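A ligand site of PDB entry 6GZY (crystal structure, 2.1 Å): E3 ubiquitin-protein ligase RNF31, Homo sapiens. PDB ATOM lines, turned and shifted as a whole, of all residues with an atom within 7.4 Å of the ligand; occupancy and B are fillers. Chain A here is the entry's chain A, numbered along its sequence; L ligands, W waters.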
ATOM      1  N   ILE A  20      28.200 -19.734 -15.837  1.00  0.00           N
ATOM      2  CA  ILE A  20      27.436 -19.700 -17.074  1.00  0.00           C
ATOM      3  C   ILE A  20      27.825 -18.433 -17.822  1.00  0.00           C
ATOM      4  O   ILE A  20      27.746 -17.333 -17.280  1.00  0.00           O
ATOM      5  CB  ILE A  20      25.916 -19.735 -16.807  1.00  0.00           C
ATOM      6  CG1 ILE A  20      25.555 -21.051 -16.103  1.00  0.00           C
ATOM      7  CG2 ILE A  20      25.138 -19.566 -18.108  1.00  0.00           C
ATOM      8  CD1 ILE A  20      24.104 -21.164 -15.696  1.00  0.00           C
ATOM      9  N   PHE A  27      28.655 -12.249 -21.059  1.00  0.00           N
ATOM     10  CA  PHE A  27      28.567 -11.959 -19.637  1.00  0.00           C
ATOM     11  C   PHE A  27      28.663 -13.254 -18.834  1.00  0.00           C
ATOM     12  O   PHE A  27      28.094 -14.279 -19.218  1.00  0.00           O
ATOM     13  CB  PHE A  27      27.251 -11.232 -19.322  1.00  0.00           C
ATOM     14  CG  PHE A  27      27.237 -10.581 -17.977  1.00  0.00           C
ATOM     15  CD1 PHE A  27      27.835  -9.343 -17.784  1.00  0.00           C
ATOM     16  CD2 PHE A  27      26.625 -11.194 -16.890  1.00  0.00           C
ATOM     17  CE1 PHE A  27      27.824  -8.732 -16.542  1.00  0.00           C
ATOM     18  CE2 PHE A  27      26.606 -10.589 -15.645  1.00  0.00           C
ATOM     19  CZ  PHE A  27      27.213  -9.352 -15.473  1.00  0.00           C
ATOM     20  N   TYR A  29      28.079 -15.413 -15.427  1.00  0.00           N
ATOM     21  CA  TYR A  29      27.329 -15.604 -14.198  1.00  0.00           C
ATOM     22  C   TYR A  29      27.963 -16.740 -13.401  1.00  0.00           C
ATOM     23  O   TYR A  29      28.300 -17.787 -13.969  1.00  0.00           O
ATOM     24  CB  TYR A  29      25.862 -15.934 -14.480  1.00  0.00           C
ATOM     25  CG  TYR A  29      25.134 -14.945 -15.372  1.00  0.00           C
ATOM     26  CD1 TYR A  29      25.170 -15.077 -16.749  1.00  0.00           C
ATOM     27  CD2 TYR A  29      24.417 -13.886 -14.828  1.00  0.00           C
ATOM     28  CE1 TYR A  29      24.507 -14.188 -17.578  1.00  0.00           C
ATOM     29  CE2 TYR A  29      23.746 -12.983 -15.642  1.00  0.00           C
ATOM     30  CZ  TYR A  29      23.794 -13.146 -17.017  1.00  0.00           C
ATOM     31  OH  TYR A  29      23.131 -12.251 -17.828  1.00  0.00           O
ATOM     32  N   LEU A  31      26.947 -19.172 -11.348  1.00  0.00           N
ATOM     33  CA  LEU A  31      25.756 -19.885 -10.924  1.00  0.00           C
ATOM     34  C   LEU A  31      25.846 -21.339 -11.359  1.00  0.00           C
ATOM     35  O   LEU A  31      26.434 -21.665 -12.398  1.00  0.00           O
ATOM     36  CB  LEU A  31      24.486 -19.255 -11.505  1.00  0.00           C
ATOM     37  CG  LEU A  31      24.105 -17.889 -10.945  1.00  0.00           C
ATOM     38  CD1 LEU A  31      23.105 -17.186 -11.849  1.00  0.00           C
ATOM     39  CD2 LEU A  31      23.534 -18.034  -9.536  1.00  0.00           C
ATOM     40  N   ALA A  32      25.250 -22.216 -10.554  1.00  0.00           N
ATOM     41  CA  ALA A  32      25.069 -23.610 -10.912  1.00  0.00           C
ATOM     42  C   ALA A  32      23.784 -23.784 -11.703  1.00  0.00           C
ATOM     43  O   ALA A  32      22.854 -22.989 -11.609  1.00  0.00           O
ATOM     44  CB  ALA A  32      25.029 -24.483  -9.655  1.00  0.00           C
ATOM     45  N   ARG A  33      23.746 -24.854 -12.497  1.00  0.00           N
ATOM     46  CA  ARG A  33      22.593 -25.142 -13.347  1.00  0.00           C
ATOM     47  C   ARG A  33      21.563 -26.009 -12.654  1.00  0.00           C
ATOM     48  O   ARG A  33      20.368 -25.886 -12.947  1.00  0.00           O
ATOM     49  CB  ARG A  33      23.042 -25.839 -14.631  1.00  0.00           C
ATOM     50  CG  ARG A  33      24.088 -25.059 -15.429  1.00  0.00           C
ATOM     51  CD  ARG A  33      25.138 -25.982 -16.007  1.00  0.00           C
ATOM     52  NE  ARG A  33      25.912 -25.341 -17.058  1.00  0.00           N
ATOM     53  CZ  ARG A  33      26.960 -24.547 -16.851  1.00  0.00           C
ATOM     54  NH1 ARG A  33      27.595 -24.003 -17.878  1.00  0.00           N
ATOM     55  NH2 ARG A  33      27.360 -24.293 -15.608  1.00  0.00           N
ATOM     56  N   GLY A  34      21.982 -26.882 -11.740  1.00  0.00           N
ATOM     57  CA  GLY A  34      21.093 -27.882 -11.174  1.00  0.00           C
ATOM     58  C   GLY A  34      20.420 -28.668 -12.278  1.00  0.00           C
ATOM     59  O   GLY A  34      21.098 -29.242 -13.142  1.00  0.00           O
ATOM     60  N   GLY A  35      19.089 -28.676 -12.286  1.00  0.00           N
ATOM     61  CA  GLY A  35      18.331 -29.245 -13.370  1.00  0.00           C
ATOM     62  C   GLY A  35      17.625 -28.226 -14.241  1.00  0.00           C
ATOM     63  O   GLY A  35      16.845 -28.609 -15.109  1.00  0.00           O
ATOM     64  N   CYS A  36      17.900 -26.938 -14.044  1.00  0.00           N
ATOM     65  CA  CYS A  36      17.255 -25.871 -14.803  1.00  0.00           C
ATOM     66  C   CYS A  36      18.102 -25.556 -16.035  1.00  0.00           C
ATOM     67  O   CYS A  36      19.207 -25.035 -15.913  1.00  0.00           O
ATOM     68  CB  CYS A  36      17.077 -24.632 -13.941  1.00  0.00           C
ATOM     69  SG  CYS A  36      16.160 -23.309 -14.744  1.00  0.00           S
ATOM     70  N   MET A  37      17.569 -25.883 -17.210  1.00  0.00           N
ATOM     71  CA  MET A  37      18.318 -25.729 -18.457  1.00  0.00           C
ATOM     72  C   MET A  37      18.007 -24.427 -19.193  1.00  0.00           C
ATOM     73  O   MET A  37      18.800 -24.020 -20.044  1.00  0.00           O
ATOM     74  CB  MET A  37      18.027 -26.905 -19.398  1.00  0.00           C
ATOM     75  CG  MET A  37      18.205 -28.278 -18.766  1.00  0.00           C
ATOM     76  SD  MET A  37      19.748 -28.471 -17.845  1.00  0.00           S
ATOM     77  CE  MET A  37      20.948 -27.966 -19.069  1.00  0.00           C
ATOM     78  N   HIS A  38      16.887 -23.775 -18.886  1.00  0.00           N
ATOM     79  CA  HIS A  38      16.493 -22.544 -19.564  1.00  0.00           C
ATOM     80  C   HIS A  38      17.155 -21.358 -18.876  1.00  0.00           C
ATOM     81  O   HIS A  38      16.804 -21.021 -17.738  1.00  0.00           O
ATOM     82  CB  HIS A  38      14.983 -22.388 -19.566  1.00  0.00           C
ATOM     83  CG  HIS A  38      14.510 -21.102 -20.171  1.00  0.00           C
ATOM     84  ND1 HIS A  38      13.717 -20.203 -19.480  1.00  0.00           N
ATOM     85  CD2 HIS A  38      14.727 -20.565 -21.388  1.00  0.00           C
ATOM     86  CE1 HIS A  38      13.468 -19.165 -20.261  1.00  0.00           C
ATOM     87  NE2 HIS A  38      14.066 -19.356 -21.419  1.00  0.00           N
ATOM     88  N   PHE A  39      18.105 -20.725 -19.554  1.00  0.00           N
ATOM     89  CA  PHE A  39      18.793 -19.562 -19.018  1.00  0.00           C
ATOM     90  C   PHE A  39      18.477 -18.344 -19.871  1.00  0.00           C
ATOM     91  O   PHE A  39      18.452 -18.419 -21.111  1.00  0.00           O
ATOM     92  CB  PHE A  39      20.306 -19.783 -18.969  1.00  0.00           C
ATOM     93  CG  PHE A  39      21.015 -18.815 -18.075  1.00  0.00           C
ATOM     94  CD1 PHE A  39      21.442 -17.587 -18.549  1.00  0.00           C
ATOM     95  CD2 PHE A  39      21.255 -19.136 -16.749  1.00  0.00           C
ATOM     96  CE1 PHE A  39      22.094 -16.702 -17.721  1.00  0.00           C
ATOM     97  CE2 PHE A  39      21.907 -18.248 -15.911  1.00  0.00           C
ATOM     98  CZ  PHE A  39      22.327 -17.029 -16.392  1.00  0.00           C
ATOM     99  N   HIS A  40      18.217 -17.226 -19.211  1.00  0.00           N
ATOM    100  CA  HIS A  40      17.880 -15.960 -19.869  1.00  0.00           C
ATOM    101  C   HIS A  40      18.865 -14.901 -19.403  1.00  0.00           C
ATOM    102  O   HIS A  40      18.929 -14.589 -18.212  1.00  0.00           O
ATOM    103  CB  HIS A  40      16.446 -15.556 -19.558  1.00  0.00           C
ATOM    104  CG  HIS A  40      16.065 -14.219 -20.117  1.00  0.00           C
ATOM    105  ND1 HIS A  40      16.433 -13.037 -19.520  1.00  0.00           N
ATOM    106  CD2 HIS A  40      15.342 -13.881 -21.214  1.00  0.00           C
ATOM    107  CE1 HIS A  40      15.954 -12.018 -20.224  1.00  0.00           C
ATOM    108  NE2 HIS A  40      15.297 -12.512 -21.260  1.00  0.00           N
ATOM    109  N   CYS A  41      19.651 -14.357 -20.329  1.00  0.00           N
ATOM    110  CA  CYS A  41      20.674 -13.370 -19.984  1.00  0.00           C
ATOM    111  C   CYS A  41      20.034 -12.020 -19.693  1.00  0.00           C
ATOM    112  O   CYS A  41      19.323 -11.460 -20.534  1.00  0.00           O
ATOM    113  CB  CYS A  41      21.693 -13.236 -21.109  1.00  0.00           C
ATOM    114  SG  CYS A  41      23.009 -12.022 -20.803  1.00  0.00           S
ATOM    115  N   THR A  42      20.319 -11.480 -18.512  1.00  0.00           N
ATOM    116  CA  THR A  42      19.839 -10.150 -18.156  1.00  0.00           C
ATOM    117  C   THR A  42      20.356  -9.095 -19.119  1.00  0.00           C
ATOM    118  O   THR A  42      19.626  -8.165 -19.482  1.00  0.00           O
ATOM    119  CB  THR A  42      20.277  -9.798 -16.736  1.00  0.00           C
ATOM    120  OG1 THR A  42      19.786 -10.788 -15.820  1.00  0.00           O
ATOM    121  CG2 THR A  42      19.754  -8.431 -16.331  1.00  0.00           C
ATOM    122  N   GLN A  43      21.621  -9.206 -19.517  1.00  0.00           N
ATOM    123  CA  GLN A  43      22.264  -8.114 -20.233  1.00  0.00           C
ATOM    124  C   GLN A  43      21.758  -7.997 -21.668  1.00  0.00           C
ATOM    125  O   GLN A  43      21.544  -6.877 -22.158  1.00  0.00           O
ATOM    126  CB  GLN A  43      23.779  -8.303 -20.218  1.00  0.00           C
ATOM    127  CG  GLN A  43      24.327  -8.655 -18.851  1.00  0.00           C
ATOM    128  CD  GLN A  43      23.948  -7.645 -17.786  1.00  0.00           C
ATOM    129  OE1 GLN A  43      23.535  -6.524 -18.087  1.00  0.00           O
ATOM    130  NE2 GLN A  43      24.082  -8.041 -16.530  1.00  0.00           N
ATOM    131  N   HIS A  46      19.205 -12.856 -24.255  1.00  0.00           N
ATOM    132  CA  HIS A  46      19.358 -14.077 -25.017  1.00  0.00           C
ATOM    133  C   HIS A  46      18.911 -15.272 -24.169  1.00  0.00           C
ATOM    134  O   HIS A  46      19.194 -15.342 -22.974  1.00  0.00           O
ATOM    135  CB  HIS A  46      20.814 -14.236 -25.456  1.00  0.00           C
ATOM    136  CG  HIS A  46      21.084 -15.457 -26.280  1.00  0.00           C
ATOM    137  ND1 HIS A  46      20.501 -15.680 -27.507  1.00  0.00           N
ATOM    138  CD2 HIS A  46      21.906 -16.516 -26.057  1.00  0.00           C
ATOM    139  CE1 HIS A  46      20.930 -16.825 -28.002  1.00  0.00           C
ATOM    140  NE2 HIS A  46      21.782 -17.353 -27.138  1.00  0.00           N
ATOM    141  N   PHE A  48      19.048 -19.382 -23.867  1.00  0.00           N
ATOM    142  CA  PHE A  48      19.875 -20.479 -24.339  1.00  0.00           C
ATOM    143  C   PHE A  48      19.905 -21.592 -23.297  1.00  0.00           C
ATOM    144  O   PHE A  48      19.527 -21.391 -22.138  1.00  0.00           O
ATOM    145  CB  PHE A  48      21.313 -20.005 -24.620  1.00  0.00           C
ATOM    146  CG  PHE A  48      22.022 -19.477 -23.413  1.00  0.00           C
ATOM    147  CD1 PHE A  48      21.821 -18.166 -22.989  1.00  0.00           C
ATOM    148  CD2 PHE A  48      22.898 -20.274 -22.690  1.00  0.00           C
ATOM    149  CE1 PHE A  48      22.483 -17.675 -21.865  1.00  0.00           C
ATOM    150  CE2 PHE A  48      23.552 -19.793 -21.573  1.00  0.00           C
ATOM    151  CZ  PHE A  48      23.338 -18.486 -21.159  1.00  0.00           C
ATOM    152  N   CYS A  49      20.352 -22.766 -23.726  1.00  0.00           N
ATOM    153  CA  CYS A  49      20.507 -23.903 -22.822  1.00  0.00           C
ATOM    154  C   CYS A  49      21.806 -23.767 -22.048  1.00  0.00           C
ATOM    155  O   CYS A  49      22.880 -23.696 -22.652  1.00  0.00           O
ATOM    156  CB  CYS A  49      20.473 -25.220 -23.583  1.00  0.00           C
ATOM    157  SG  CYS A  49      20.716 -26.675 -22.530  1.00  0.00           S
ATOM    158  N   SER A  50      21.718 -23.764 -20.718  1.00  0.00           N
ATOM    159  CA  SER A  50      22.901 -23.645 -19.887  1.00  0.00           C
ATOM    160  C   SER A  50      23.791 -24.887 -19.945  1.00  0.00           C
ATOM    161  O   SER A  50      24.888 -24.857 -19.371  1.00  0.00           O
ATOM    162  CB  SER A  50      22.485 -23.388 -18.439  1.00  0.00           C
ATOM    163  OG  SER A  50      21.716 -24.468 -17.924  1.00  0.00           O
ATOM    164  N   GLY A  51      23.366 -25.948 -20.612  1.00  0.00           N
ATOM    165  CA  GLY A  51      24.158 -27.166 -20.661  1.00  0.00           C
ATOM    166  C   GLY A  51      24.954 -27.301 -21.943  1.00  0.00           C
ATOM    167  O   GLY A  51      26.073 -27.836 -21.930  1.00  0.00           O
ATOM    168  N   GLU A 124      21.925 -20.022  -5.136  1.00  0.00           N
ATOM    169  CA  GLU A 124      21.039 -19.702  -6.241  1.00  0.00           C
ATOM    170  C   GLU A 124      20.350 -18.363  -5.968  1.00  0.00           C
ATOM    171  O   GLU A 124      20.566 -17.732  -4.932  1.00  0.00           O
ATOM    172  CB  GLU A 124      19.992 -20.812  -6.441  1.00  0.00           C
ATOM    173  CG  GLU A 124      20.486 -22.220  -6.142  1.00  0.00           C
ATOM    174  CD  GLU A 124      19.365 -23.258  -6.169  1.00  0.00           C
ATOM    175  OE1 GLU A 124      18.368 -23.034  -6.895  1.00  0.00           O
ATOM    176  OE2 GLU A 124      19.482 -24.280  -5.462  1.00  0.00           O
ATOM    177  N   GLN A 125      19.511 -17.946  -6.917  1.00  0.00           N
ATOM    178  CA  GLN A 125      18.737 -16.716  -6.776  1.00  0.00           C
ATOM    179  C   GLN A 125      17.288 -17.028  -6.430  1.00  0.00           C
ATOM    180  O   GLN A 125      16.899 -18.186  -6.295  1.00  0.00           O
ATOM    181  CB  GLN A 125      18.763 -15.908  -8.083  1.00  0.00           C
ATOM    182  CG  GLN A 125      20.090 -15.288  -8.456  1.00  0.00           C
ATOM    183  N   GLU A 155      24.712 -32.791 -11.751  1.00  0.00           N
ATOM    184  CA  GLU A 155      25.411 -31.746 -12.501  1.00  0.00           C
ATOM    185  C   GLU A 155      26.915 -31.886 -12.344  1.00  0.00           C
ATOM    186  O   GLU A 155      27.667 -31.746 -13.317  1.00  0.00           O
ATOM    187  CB  GLU A 155      24.957 -30.356 -12.028  1.00  0.00           C
ATOM    188  CG  GLU A 155      25.625 -29.193 -12.771  1.00  0.00           C
ATOM    189  CD  GLU A 155      25.292 -27.825 -12.179  1.00  0.00           C
ATOM    190  OE1 GLU A 155      25.825 -26.815 -12.694  1.00  0.00           O
ATOM    191  OE2 GLU A 155      24.486 -27.750 -11.229  1.00  0.00           O
HETATM  192  C1  LIG L   1      18.218 -19.231 -13.979  1.00  0.00           C
HETATM  193  O1  LIG L   1      18.789 -19.864 -13.092  1.00  0.00           O
HETATM  194  C2  LIG L   1      16.582 -21.057 -14.299  1.00  0.00           C
HETATM  195  C3  LIG L   1      19.580 -15.288 -14.910  1.00  0.00           C
HETATM  196  C4  LIG L   1      20.632 -14.873 -12.822  1.00  0.00           C
HETATM  197  C5  LIG L   1      18.394 -17.260 -15.656  1.00  0.00           C
HETATM  198  C6  LIG L   1      20.792 -13.649 -13.731  1.00  0.00           C
HETATM  199  C7  LIG L   1      20.113 -13.903 -15.088  1.00  0.00           C
HETATM  200  C8  LIG L   1      17.404 -22.274 -14.767  1.00  0.00           C
HETATM  201  C9  LIG L   1      18.551 -21.955 -15.714  1.00  0.00           C
HETATM  202  C10 LIG L   1      21.305 -21.255 -13.406  1.00  0.00           C
HETATM  203  C11 LIG L   1      18.696 -17.834 -14.347  1.00  0.00           C
HETATM  204  C12 LIG L   1      19.394 -17.121 -13.406  1.00  0.00           C
HETATM  205  C13 LIG L   1      19.850 -15.820 -13.672  1.00  0.00           C
HETATM  206  N1  LIG L   1      18.883 -15.974 -15.861  1.00  0.00           N
HETATM  207  N2  LIG L   1      17.148 -19.728 -14.616  1.00  0.00           N
HETATM  208  O2  LIG L   1      17.770 -17.837 -16.551  1.00  0.00           O
HETATM  209  O3  LIG L   1      20.890 -22.547 -15.799  1.00  0.00           O
HETATM  210  O4  LIG L   1      20.070 -21.911 -13.791  1.00  0.00           O
HETATM  211  O   HOH W   1      16.045 -19.228 -12.023  1.00  0.00           O
HETATM  212  O   HOH W   2      15.161 -18.004 -16.807  1.00  0.00           O
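CD1 of Ile 20 touches O3 of the ligand, 3.5 Å away.
CE2 of Tyr 29 touches C6 of the ligand, at 3.6 Å.
Leu 31 touches the ligand.
Ala 32 touches the ligand.
Arg 33 touches the ligand.
CA of Phe 39 touches O2 of the ligand, 3.2 Å away.
OG1 of Thr 42 touches C7 of the ligand, 3.2 Å away.
The nearest printed residue that does not touch the ligand is Met 37 (4.3 Å).
A carbon (C8) of the ligand is covalently linked to the side-chain sulfur of Cys 36 (1.6 Å).
The backbone NH of His 40 sits at hydrogen-bond distance from an oxygen (O2) of the ligand, at 2.8 Å.
The backbone carbonyl oxygen of His 40 lies within hydrogen-bond range of a nitrogen (N1) of the ligand (2.7 Å).
O of His 38 lies close to N2 of the ligand, 3.4 Å away.
O3 of the ligand is in hydrogen-bond range of OG of Ser 50 (3.0 Å).
The backbone carbonyl oxygen of Cys 36 sits at hydrogen-bond distance from the side-chain hydroxyl of Ser 50, 3.3 Å away.
The backbone carbonyl oxygen (O) of Ser 50 is in hydrogen-bond range of the guanidinium group (NE) of Arg 33, at 2.6 Å.
The backbone NH (N) of Ser 50 sits at hydrogen-bond distance from the backbone carbonyl oxygen (O) of Met 37.
The backbone NH of Phe 48 sits at hydrogen-bond distance from the backbone carbonyl oxygen of Phe 39.
N of Thr 42 sits at hydrogen-bond distance from OH of Tyr 29 (3.0 Å).
The backbone NH (N) of Tyr 29 sits at hydrogen-bond distance from the backbone carbonyl oxygen (O) of Ile 20 (2.7 Å).
The side-chain hydroxyl (OH) of Tyr 29 lies close to the side-chain sulfur (SG) of Cys 41, 3.0 Å away.
The backbone NH of Arg 33 is in hydrogen-bond range of the side-chain carboxylate of Glu 155, 2.9 Å away.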
